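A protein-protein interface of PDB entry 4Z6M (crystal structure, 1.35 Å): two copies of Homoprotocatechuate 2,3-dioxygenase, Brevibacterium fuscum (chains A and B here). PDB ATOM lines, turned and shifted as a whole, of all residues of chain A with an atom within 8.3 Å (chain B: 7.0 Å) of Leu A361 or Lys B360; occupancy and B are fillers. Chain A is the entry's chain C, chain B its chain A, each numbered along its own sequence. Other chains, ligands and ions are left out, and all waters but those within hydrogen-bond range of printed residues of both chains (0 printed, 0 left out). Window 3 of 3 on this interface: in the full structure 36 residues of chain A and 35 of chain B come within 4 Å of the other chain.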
ATOM      1  N   VAL A 300     -28.089   2.163  15.400  1.00  0.00           N
ATOM      2  CA  VAL A 300     -29.238   2.048  14.498  1.00  0.00           C
ATOM      3  C   VAL A 300     -30.053   3.326  14.596  1.00  0.00           C
ATOM      4  O   VAL A 300     -30.548   3.675  15.652  1.00  0.00           O
ATOM      5  CB  VAL A 300     -30.112   0.812  14.778  1.00  0.00           C
ATOM      6  CG1 VAL A 300     -31.299   0.783  13.828  1.00  0.00           C
ATOM      7  CG2 VAL A 300     -29.296  -0.461  14.697  1.00  0.00           C
ATOM      8  N   VAL A 301     -30.168   4.010  13.460  1.00  0.00           N
ATOM      9  CA  VAL A 301     -30.920   5.253  13.312  1.00  0.00           C
ATOM     10  C   VAL A 301     -32.374   5.078  13.795  1.00  0.00           C
ATOM     11  O   VAL A 301     -33.034   4.111  13.419  1.00  0.00           O
ATOM     12  CB  VAL A 301     -30.852   5.685  11.819  1.00  0.00           C
ATOM     13  CG1 VAL A 301     -31.752   6.869  11.510  1.00  0.00           C
ATOM     14  CG2 VAL A 301     -29.410   5.983  11.417  1.00  0.00           C
ATOM     15  N   PRO A 302     -32.876   5.993  14.653  1.00  0.00           N
ATOM     16  CA  PRO A 302     -34.206   5.726  15.232  1.00  0.00           C
ATOM     17  C   PRO A 302     -35.343   5.600  14.209  1.00  0.00           C
ATOM     18  O   PRO A 302     -36.263   4.796  14.386  1.00  0.00           O
ATOM     19  CB  PRO A 302     -34.449   6.901  16.193  1.00  0.00           C
ATOM     20  CG  PRO A 302     -33.247   7.785  16.096  1.00  0.00           C
ATOM     21  CD  PRO A 302     -32.193   7.143  15.273  1.00  0.00           C
ATOM     22  N   SER A 303     -35.234   6.320  13.105  1.00  0.00           N
ATOM     23  CA  SER A 303     -36.263   6.255  12.079  1.00  0.00           C
ATOM     24  C   SER A 303     -36.347   4.854  11.490  1.00  0.00           C
ATOM     25  O   SER A 303     -37.375   4.474  10.939  1.00  0.00           O
ATOM     26  CB  SER A 303     -36.010   7.259  10.961  1.00  0.00           C
ATOM     27  OG  SER A 303     -34.776   7.026  10.310  1.00  0.00           O
ATOM     28  N   TYR A 305     -36.369   2.135  13.120  1.00  0.00           N
ATOM     29  CA  TYR A 305     -37.317   1.423  13.955  1.00  0.00           C
ATOM     30  C   TYR A 305     -38.725   1.961  13.881  1.00  0.00           C
ATOM     31  O   TYR A 305     -39.645   1.236  14.250  1.00  0.00           O
ATOM     32  CB  TYR A 305     -36.866   1.485  15.411  1.00  0.00           C
ATOM     33  CG  TYR A 305     -35.641   0.649  15.718  1.00  0.00           C
ATOM     34  CD1 TYR A 305     -35.611  -0.712  15.416  1.00  0.00           C
ATOM     35  CD2 TYR A 305     -34.519   1.209  16.290  1.00  0.00           C
ATOM     36  CE1 TYR A 305     -34.505  -1.484  15.701  1.00  0.00           C
ATOM     37  CE2 TYR A 305     -33.406   0.432  16.592  1.00  0.00           C
ATOM     38  CZ  TYR A 305     -33.400  -0.913  16.281  1.00  0.00           C
ATOM     39  OH  TYR A 305     -32.276  -1.685  16.566  1.00  0.00           O
ATOM     40  N   THR A 306     -38.913   3.232  13.523  1.00  0.00           N
ATOM     41  CA  THR A 306     -40.228   3.873  13.660  1.00  0.00           C
ATOM     42  C   THR A 306     -40.976   4.111  12.342  1.00  0.00           C
ATOM     43  O   THR A 306     -42.190   4.103  12.322  1.00  0.00           O
ATOM     44  CB  THR A 306     -40.156   5.205  14.436  1.00  0.00           C
ATOM     45  OG1 THR A 306     -39.398   6.155  13.705  1.00  0.00           O
ATOM     46  CG2 THR A 306     -39.535   5.029  15.811  1.00  0.00           C
ATOM     47  N   LEU A 330     -36.223  -0.656  19.703  1.00  0.00           N
ATOM     48  CA  LEU A 330     -35.676   0.674  19.964  1.00  0.00           C
ATOM     49  C   LEU A 330     -35.572   0.935  21.463  1.00  0.00           C
ATOM     50  O   LEU A 330     -34.519   1.282  21.983  1.00  0.00           O
ATOM     51  CB  LEU A 330     -36.533   1.750  19.300  1.00  0.00           C
ATOM     52  CG  LEU A 330     -36.055   3.207  19.440  1.00  0.00           C
ATOM     53  CD1 LEU A 330     -36.663   4.040  18.321  1.00  0.00           C
ATOM     54  CD2 LEU A 330     -36.404   3.831  20.789  1.00  0.00           C
ATOM     55  N   GLU A 331     -36.678   0.763  22.164  1.00  0.00           N
ATOM     56  CA  GLU A 331     -36.700   1.138  23.592  1.00  0.00           C
ATOM     57  C   GLU A 331     -35.728   0.314  24.435  1.00  0.00           C
ATOM     58  O   GLU A 331     -35.031   0.872  25.299  1.00  0.00           O
ATOM     59  CB  GLU A 331     -38.111   1.046  24.154  1.00  0.00           C
ATOM     60  CG  GLU A 331     -39.066   2.058  23.544  1.00  0.00           C
ATOM     61  CD  GLU A 331     -38.768   3.509  23.931  1.00  0.00           C
ATOM     62  OE1 GLU A 331     -37.915   3.763  24.812  1.00  0.00           O
ATOM     63  OE2 GLU A 331     -39.397   4.421  23.343  1.00  0.00           O
ATOM     64  N   THR A 333     -32.944  -1.129  23.574  1.00  0.00           N
ATOM     65  CA  THR A 333     -31.551  -1.049  23.175  1.00  0.00           C
ATOM     66  C   THR A 333     -30.993   0.376  23.232  1.00  0.00           C
ATOM     67  O   THR A 333     -29.871   0.552  23.694  1.00  0.00           O
ATOM     68  CB  THR A 333     -31.322  -1.607  21.757  1.00  0.00           C
ATOM     69  OG1 THR A 333     -32.037  -0.854  20.774  1.00  0.00           O
ATOM     70  CG2 THR A 333     -31.701  -3.083  21.687  1.00  0.00           C
ATOM     71  N   ILE A 334     -31.732   1.378  22.728  1.00  0.00           N
ATOM     72  CA  ILE A 334     -31.199   2.741  22.600  1.00  0.00           C
ATOM     73  C   ILE A 334     -32.065   3.819  23.276  1.00  0.00           C
ATOM     74  O   ILE A 334     -31.679   4.979  23.291  1.00  0.00           O
ATOM     75  CB  ILE A 334     -30.917   3.130  21.131  1.00  0.00           C
ATOM     76  CG1 ILE A 334     -32.172   3.071  20.244  1.00  0.00           C
ATOM     77  CG2 ILE A 334     -29.842   2.232  20.551  1.00  0.00           C
ATOM     78  CD1 ILE A 334     -31.981   3.654  18.853  1.00  0.00           C
ATOM     79  N   GLY A 335     -33.207   3.430  23.826  1.00  0.00           N
ATOM     80  CA  GLY A 335     -34.051   4.330  24.583  1.00  0.00           C
ATOM     81  C   GLY A 335     -33.523   4.570  25.981  1.00  0.00           C
ATOM     82  O   GLY A 335     -32.507   3.987  26.411  1.00  0.00           O
ATOM     83  N   ALA A 336     -34.228   5.432  26.699  1.00  0.00           N
ATOM     84  CA  ALA A 336     -33.782   5.884  28.008  1.00  0.00           C
ATOM     85  C   ALA A 336     -33.598   4.749  29.007  1.00  0.00           C
ATOM     86  O   ALA A 336     -32.760   4.868  29.897  1.00  0.00           O
ATOM     87  CB  ALA A 336     -34.752   6.914  28.582  1.00  0.00           C
ATOM     88  N   ASP A 337     -34.394   3.678  28.891  1.00  0.00           N
ATOM     89  CA  ASP A 337     -34.276   2.528  29.793  1.00  0.00           C
ATOM     90  C   ASP A 337     -33.670   1.283  29.119  1.00  0.00           C
ATOM     91  O   ASP A 337     -33.734   0.173  29.652  1.00  0.00           O
ATOM     92  CB  ASP A 337     -35.636   2.197  30.412  1.00  0.00           C
ATOM     93  CG  ASP A 337     -36.244   3.376  31.152  1.00  0.00           C
ATOM     94  OD1 ASP A 337     -35.503   4.104  31.858  1.00  0.00           O
ATOM     95  OD2 ASP A 337     -37.465   3.573  31.023  1.00  0.00           O
ATOM     96  N   GLY A 338     -33.060   1.491  27.960  1.00  0.00           N
ATOM     97  CA  GLY A 338     -32.459   0.398  27.186  1.00  0.00           C
ATOM     98  C   GLY A 338     -30.988   0.202  27.473  1.00  0.00           C
ATOM     99  O   GLY A 338     -30.361   0.983  28.218  1.00  0.00           O
ATOM    100  N   GLY A 353     -29.043   3.614  28.296  1.00  0.00           N
ATOM    101  CA  GLY A 353     -29.886   4.793  28.096  1.00  0.00           C
ATOM    102  C   GLY A 353     -29.444   5.690  26.960  1.00  0.00           C
ATOM    103  O   GLY A 353     -29.802   6.865  26.925  1.00  0.00           O
ATOM    104  N   GLN A 354     -28.688   5.125  26.021  1.00  0.00           N
ATOM    105  CA  GLN A 354     -28.253   5.841  24.850  1.00  0.00           C
ATOM    106  C   GLN A 354     -27.729   4.862  23.831  1.00  0.00           C
ATOM    107  O   GLN A 354     -27.652   3.675  24.092  1.00  0.00           O
ATOM    108  CB  GLN A 354     -27.189   6.866  25.200  1.00  0.00           C
ATOM    109  CG  GLN A 354     -25.924   6.297  25.797  1.00  0.00           C
ATOM    110  CD  GLN A 354     -25.051   7.378  26.409  1.00  0.00           C
ATOM    111  OE1 GLN A 354     -25.434   8.548  26.473  1.00  0.00           O
ATOM    112  NE2 GLN A 354     -23.892   6.983  26.889  1.00  0.00           N
ATOM    113  N   ALA A 355     -27.418   5.363  22.651  1.00  0.00           N
ATOM    114  CA  ALA A 355     -26.884   4.521  21.585  1.00  0.00           C
ATOM    115  C   ALA A 355     -25.368   4.410  21.720  1.00  0.00           C
ATOM    116  O   ALA A 355     -24.747   5.000  22.620  1.00  0.00           O
ATOM    117  CB  ALA A 355     -27.296   5.077  20.236  1.00  0.00           C
ATOM    118  N   SER A 356     -24.778   3.642  20.812  1.00  0.00           N
ATOM    119  CA  SER A 356     -23.339   3.548  20.704  1.00  0.00           C
ATOM    120  C   SER A 356     -22.715   4.811  20.109  1.00  0.00           C
ATOM    121  O   SER A 356     -23.405   5.701  19.596  1.00  0.00           O
ATOM    122  CB  SER A 356     -23.001   2.348  19.830  1.00  0.00           C
ATOM    123  OG  SER A 356     -23.621   2.523  18.566  1.00  0.00           O
ATOM    124  N   LYS A 357     -21.390   4.862  20.179  1.00  0.00           N
ATOM    125  CA  LYS A 357     -20.536   5.852  19.513  1.00  0.00           C
ATOM    126  C   LYS A 357     -20.779   7.284  19.993  1.00  0.00           C
ATOM    127  O   LYS A 357     -20.418   8.246  19.309  1.00  0.00           O
ATOM    128  CB  LYS A 357     -20.673   5.787  17.988  1.00  0.00           C
ATOM    129  CG  LYS A 357     -20.599   4.401  17.341  1.00  0.00           C
ATOM    130  CD  LYS A 357     -19.320   3.609  17.567  1.00  0.00           C
ATOM    131  CE  LYS A 357     -19.302   2.356  16.691  1.00  0.00           C
ATOM    132  NZ  LYS A 357     -18.337   1.323  17.193  1.00  0.00           N
ATOM    133  N   GLY A 358     -21.328   7.437  21.189  1.00  0.00           N
ATOM    134  CA  GLY A 358     -21.481   8.765  21.807  1.00  0.00           C
ATOM    135  C   GLY A 358     -22.793   9.490  21.546  1.00  0.00           C
ATOM    136  O   GLY A 358     -22.918  10.666  21.884  1.00  0.00           O
ATOM    137  N   PHE A 359     -23.773   8.794  20.966  1.00  0.00           N
ATOM    138  CA  PHE A 359     -25.044   9.407  20.590  1.00  0.00           C
ATOM    139  C   PHE A 359     -26.224   8.971  21.482  1.00  0.00           C
ATOM    140  O   PHE A 359     -26.224   7.893  22.055  1.00  0.00           O
ATOM    141  CB  PHE A 359     -25.383   9.081  19.126  1.00  0.00           C
ATOM    142  CG  PHE A 359     -24.391   9.605  18.133  1.00  0.00           C
ATOM    143  CD1 PHE A 359     -24.204  10.966  17.966  1.00  0.00           C
ATOM    144  CD2 PHE A 359     -23.675   8.736  17.338  1.00  0.00           C
ATOM    145  CE1 PHE A 359     -23.280  11.438  17.051  1.00  0.00           C
ATOM    146  CE2 PHE A 359     -22.760   9.204  16.412  1.00  0.00           C
ATOM    147  CZ  PHE A 359     -22.567  10.552  16.265  1.00  0.00           C
ATOM    148  N   LYS A 360     -27.216   9.852  21.579  1.00  0.00           N
ATOM    149  CA  LYS A 360     -28.513   9.610  22.188  1.00  0.00           C
ATOM    150  C   LYS A 360     -29.572   9.824  21.118  1.00  0.00           C
ATOM    151  O   LYS A 360     -29.278  10.394  20.059  1.00  0.00           O
ATOM    152  CB  LYS A 360     -28.763  10.629  23.323  1.00  0.00           C
ATOM    153  CG  LYS A 360     -28.505  10.118  24.719  1.00  0.00           C
ATOM    154  CD  LYS A 360     -28.882  11.171  25.761  1.00  0.00           C
ATOM    155  CE  LYS A 360     -29.786  10.579  26.849  1.00  0.00           C
ATOM    156  NZ  LYS A 360     -30.194  11.528  27.934  1.00  0.00           N
ATOM    157  N   LEU A 361     -30.803   9.417  21.420  1.00  0.00           N
ATOM    158  CA  LEU A 361     -31.955   9.631  20.528  1.00  0.00           C
ATOM    159  C   LEU A 361     -32.235  11.121  20.373  1.00  0.00           C
ATOM    160  O   LEU A 361     -32.318  11.830  21.385  1.00  0.00           O
ATOM    161  CB  LEU A 361     -33.204   8.963  21.120  1.00  0.00           C
ATOM    162  CG  LEU A 361     -33.387   7.446  21.084  1.00  0.00           C
ATOM    163  CD1 LEU A 361     -34.498   7.040  22.047  1.00  0.00           C
ATOM    164  CD2 LEU A 361     -33.754   6.987  19.693  1.00  0.00           C
ATOM    165  N   GLY A 362     -32.394  11.601  19.132  1.00  0.00           N
ATOM    166  CA  GLY A 362     -32.800  12.986  18.873  1.00  0.00           C
ATOM    167  C   GLY A 362     -34.238  13.304  19.235  1.00  0.00           C
ATOM    168  O   GLY A 362     -35.017  12.411  19.582  1.00  0.00           O
ATOM    169  N   PRO B 302     -18.938  12.627  18.864  1.00  0.00           N
ATOM    170  CA  PRO B 302     -18.454  13.755  19.685  1.00  0.00           C
ATOM    171  C   PRO B 302     -17.021  13.574  20.197  1.00  0.00           C
ATOM    172  O   PRO B 302     -16.267  14.546  20.290  1.00  0.00           O
ATOM    173  CB  PRO B 302     -19.473  13.838  20.827  1.00  0.00           C
ATOM    174  CG  PRO B 302     -20.335  12.634  20.707  1.00  0.00           C
ATOM    175  CD  PRO B 302     -20.226  12.096  19.326  1.00  0.00           C
ATOM    176  N   ILE B 334     -23.136  20.291  16.061  1.00  0.00           N
ATOM    177  CA  ILE B 334     -23.934  19.190  16.630  1.00  0.00           C
ATOM    178  C   ILE B 334     -24.330  19.383  18.083  1.00  0.00           C
ATOM    179  O   ILE B 334     -25.035  18.547  18.630  1.00  0.00           O
ATOM    180  CB  ILE B 334     -23.251  17.803  16.473  1.00  0.00           C
ATOM    181  CG1 ILE B 334     -21.879  17.758  17.140  1.00  0.00           C
ATOM    182  CG2 ILE B 334     -23.092  17.447  15.007  1.00  0.00           C
ATOM    183  CD1 ILE B 334     -21.235  16.370  17.100  1.00  0.00           C
ATOM    184  N   HIS B 352     -30.954  21.228  13.522  1.00  0.00           N
ATOM    185  CA  HIS B 352     -30.879  22.267  14.535  1.00  0.00           C
ATOM    186  C   HIS B 352     -30.728  21.647  15.911  1.00  0.00           C
ATOM    187  O   HIS B 352     -31.628  20.942  16.371  1.00  0.00           O
ATOM    188  CB  HIS B 352     -32.182  23.064  14.554  1.00  0.00           C
ATOM    189  CG  HIS B 352     -32.478  23.768  13.281  1.00  0.00           C
ATOM    190  ND1 HIS B 352     -32.132  25.082  13.071  1.00  0.00           N
ATOM    191  CD2 HIS B 352     -33.108  23.353  12.157  1.00  0.00           C
ATOM    192  CE1 HIS B 352     -32.524  25.449  11.865  1.00  0.00           C
ATOM    193  NE2 HIS B 352     -33.117  24.415  11.288  1.00  0.00           N
ATOM    194  N   GLY B 353     -29.615  21.937  16.575  1.00  0.00           N
ATOM    195  CA  GLY B 353     -29.421  21.485  17.946  1.00  0.00           C
ATOM    196  C   GLY B 353     -29.267  19.979  18.087  1.00  0.00           C
ATOM    197  O   GLY B 353     -29.480  19.431  19.155  1.00  0.00           O
ATOM    198  N   GLN B 354     -28.876  19.315  17.000  1.00  0.00           N
ATOM    199  CA  GLN B 354     -28.702  17.875  17.004  1.00  0.00           C
ATOM    200  C   GLN B 354     -27.757  17.491  15.889  1.00  0.00           C
ATOM    201  O   GLN B 354     -27.395  18.328  15.062  1.00  0.00           O
ATOM    202  CB  GLN B 354     -30.047  17.166  16.863  1.00  0.00           C
ATOM    203  CG  GLN B 354     -30.885  17.557  15.664  1.00  0.00           C
ATOM    204  CD  GLN B 354     -32.304  17.003  15.761  1.00  0.00           C
ATOM    205  OE1 GLN B 354     -32.559  16.018  16.455  1.00  0.00           O
ATOM    206  NE2 GLN B 354     -33.226  17.633  15.065  1.00  0.00           N
ATOM    207  N   ALA B 355     -27.326  16.232  15.904  1.00  0.00           N
ATOM    208  CA  ALA B 355     -26.570  15.661  14.826  1.00  0.00           C
ATOM    209  C   ALA B 355     -27.480  15.193  13.711  1.00  0.00           C
ATOM    210  O   ALA B 355     -28.702  15.180  13.850  1.00  0.00           O
ATOM    211  CB  ALA B 355     -25.708  14.533  15.354  1.00  0.00           C
ATOM    212  N   SER B 356     -26.880  14.790  12.605  1.00  0.00           N
ATOM    213  CA  SER B 356     -27.617  14.204  11.510  1.00  0.00           C
ATOM    214  C   SER B 356     -28.115  12.797  11.859  1.00  0.00           C
ATOM    215  O   SER B 356     -27.709  12.197  12.871  1.00  0.00           O
ATOM    216  CB  SER B 356     -26.709  14.165  10.305  1.00  0.00           C
ATOM    217  OG  SER B 356     -25.551  13.408  10.612  1.00  0.00           O
ATOM    218  N   GLY B 358     -30.783  11.535  13.003  1.00  0.00           N
ATOM    219  CA  GLY B 358     -31.704  11.272  14.105  1.00  0.00           C
ATOM    220  C   GLY B 358     -31.101  11.254  15.497  1.00  0.00           C
ATOM    221  O   GLY B 358     -31.797  10.900  16.443  1.00  0.00           O
ATOM    222  N   PHE B 359     -29.835  11.641  15.637  1.00  0.00           N
ATOM    223  CA  PHE B 359     -29.100  11.540  16.898  1.00  0.00           C
ATOM    224  C   PHE B 359     -28.857  12.911  17.543  1.00  0.00           C
ATOM    225  O   PHE B 359     -28.703  13.909  16.857  1.00  0.00           O
ATOM    226  CB  PHE B 359     -27.761  10.835  16.693  1.00  0.00           C
ATOM    227  CG  PHE B 359     -27.894   9.420  16.225  1.00  0.00           C
ATOM    228  CD1 PHE B 359     -28.507   8.462  17.031  1.00  0.00           C
ATOM    229  CD2 PHE B 359     -27.451   9.045  14.955  1.00  0.00           C
ATOM    230  CE1 PHE B 359     -28.643   7.154  16.587  1.00  0.00           C
ATOM    231  CE2 PHE B 359     -27.575   7.737  14.521  1.00  0.00           C
ATOM    232  CZ  PHE B 359     -28.179   6.793  15.332  1.00  0.00           C
ATOM    233  N   LYS B 360     -28.825  12.927  18.872  1.00  0.00           N
ATOM    234  CA  LYS B 360     -28.296  14.028  19.686  1.00  0.00           C
ATOM    235  C   LYS B 360     -27.037  13.551  20.381  1.00  0.00           C
ATOM    236  O   LYS B 360     -26.698  12.363  20.317  1.00  0.00           O
ATOM    237  CB  LYS B 360     -29.314  14.436  20.774  1.00  0.00           C
ATOM    238  CG  LYS B 360     -30.327  15.473  20.356  1.00  0.00           C
ATOM    239  CD  LYS B 360     -31.156  15.996  21.531  1.00  0.00           C
ATOM    240  CE  LYS B 360     -31.333  15.000  22.680  1.00  0.00           C
ATOM    241  NZ  LYS B 360     -32.355  15.461  23.670  1.00  0.00           N
ATOM    242  N   LEU B 361     -26.354  14.453  21.076  1.00  0.00           N
ATOM    243  CA  LEU B 361     -25.147  14.054  21.804  1.00  0.00           C
ATOM    244  C   LEU B 361     -25.475  13.345  23.106  1.00  0.00           C
ATOM    245  O   LEU B 361     -26.335  13.791  23.844  1.00  0.00           O
ATOM    246  CB  LEU B 361     -24.258  15.265  22.052  1.00  0.00           C
ATOM    247  CG  LEU B 361     -23.767  15.919  20.745  1.00  0.00           C
ATOM    248  CD1 LEU B 361     -22.498  16.722  20.987  1.00  0.00           C
ATOM    249  CD2 LEU B 361     -23.545  14.918  19.608  1.00  0.00           C
ATOM    250  N   GLY B 362     -24.781  12.239  23.372  1.00  0.00           N
ATOM    251  CA  GLY B 362     -24.983  11.451  24.589  1.00  0.00           C
ATOM    252  C   GLY B 362     -24.336  12.075  25.817  1.00  0.00           C
ATOM    253  O   GLY B 362     -23.720  13.140  25.721  1.00  0.00           O
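The backbone NH (N) of Gly A362 is in hydrogen-bond range of the backbone carbonyl oxygen (O) of Gly B358 (2.8 Å). N of Lys B360 sits at hydrogen-bond distance from O of Lys A360, 2.8 Å away. N of Gly B362 is in hydrogen-bond range of O of Gly A358 (2.9 Å).
The backbone carbonyl oxygen (O) of Pro A302 lies within hydrogen-bond range of the side-chain hydroxyl (OG1) of Thr A306 (3.5 Å).
Val A300 touches Phe B359. O of Gly B358 touches CG of Pro A302 (3.5 Å). Leu B361 touches Gly A358. CD1 of Phe A359 touches CB of Phe B359, at 3.8 Å. Phe A359 touches Lys B360 (CA to O, 3.4 Å). CA of Phe A359 touches N of Gly B362, at 3.98 Å. Phe B359 touches Lys A360. Leu A361 touches Lys B360 (O to CE, 3.6 Å). Gly A362 touches Phe B359 (N to CA, 3.98 Å). Lys B360 touches Gly A362.
Ile A334 touches none of the printed residues of chain B. Gly A335 touches none of the printed residues of chain B. Printed residues of chain B within 4 Å of Gly A358: Pro B302 (3.5 Å), Leu B361 (3.9 Å) and Gly B362 (2.9 Å). Printed residues of chain B within 4 Å of Leu A361: Gly B358 and Lys B360. Of the printed residues of chain A, Gln B354 touches Gly A362 (3.9 Å). Of chain A, only Phe A359, Lys A360, Leu A361 and Gly A362 come within 4 Å of Lys B360. Of the printed residues of chain A, Leu B361 touches Gly A358 (3.9 Å). The nearest residue of chain A that does not touch Lys B360 is Gly A358 (4.4 Å). The nearest printed residue of chain B that does not touch Gln A354 is Leu B361 (5.9 Å).
Hydrophobic or aromatic side chains of chain A that line the printed part of chain B: Pro A302 and Phe A359. Among the printed residues, 22 pairs touch across the chains.
Phe B359 touches its own counterpart, Phe A359. Lys A360 touches its own counterpart, Lys B360. Lys A360 touches Gly B362, and with the chains exchanged Gly A362 touches Lys B360. Leu A361 touches Lys B360, but with the chains exchanged Lys A360 does not touch Leu B361 (4.02 Å). Of the 22 pairs that touch across the chains among the printed residues, 18 have their exchanged pair printed and touching as well.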
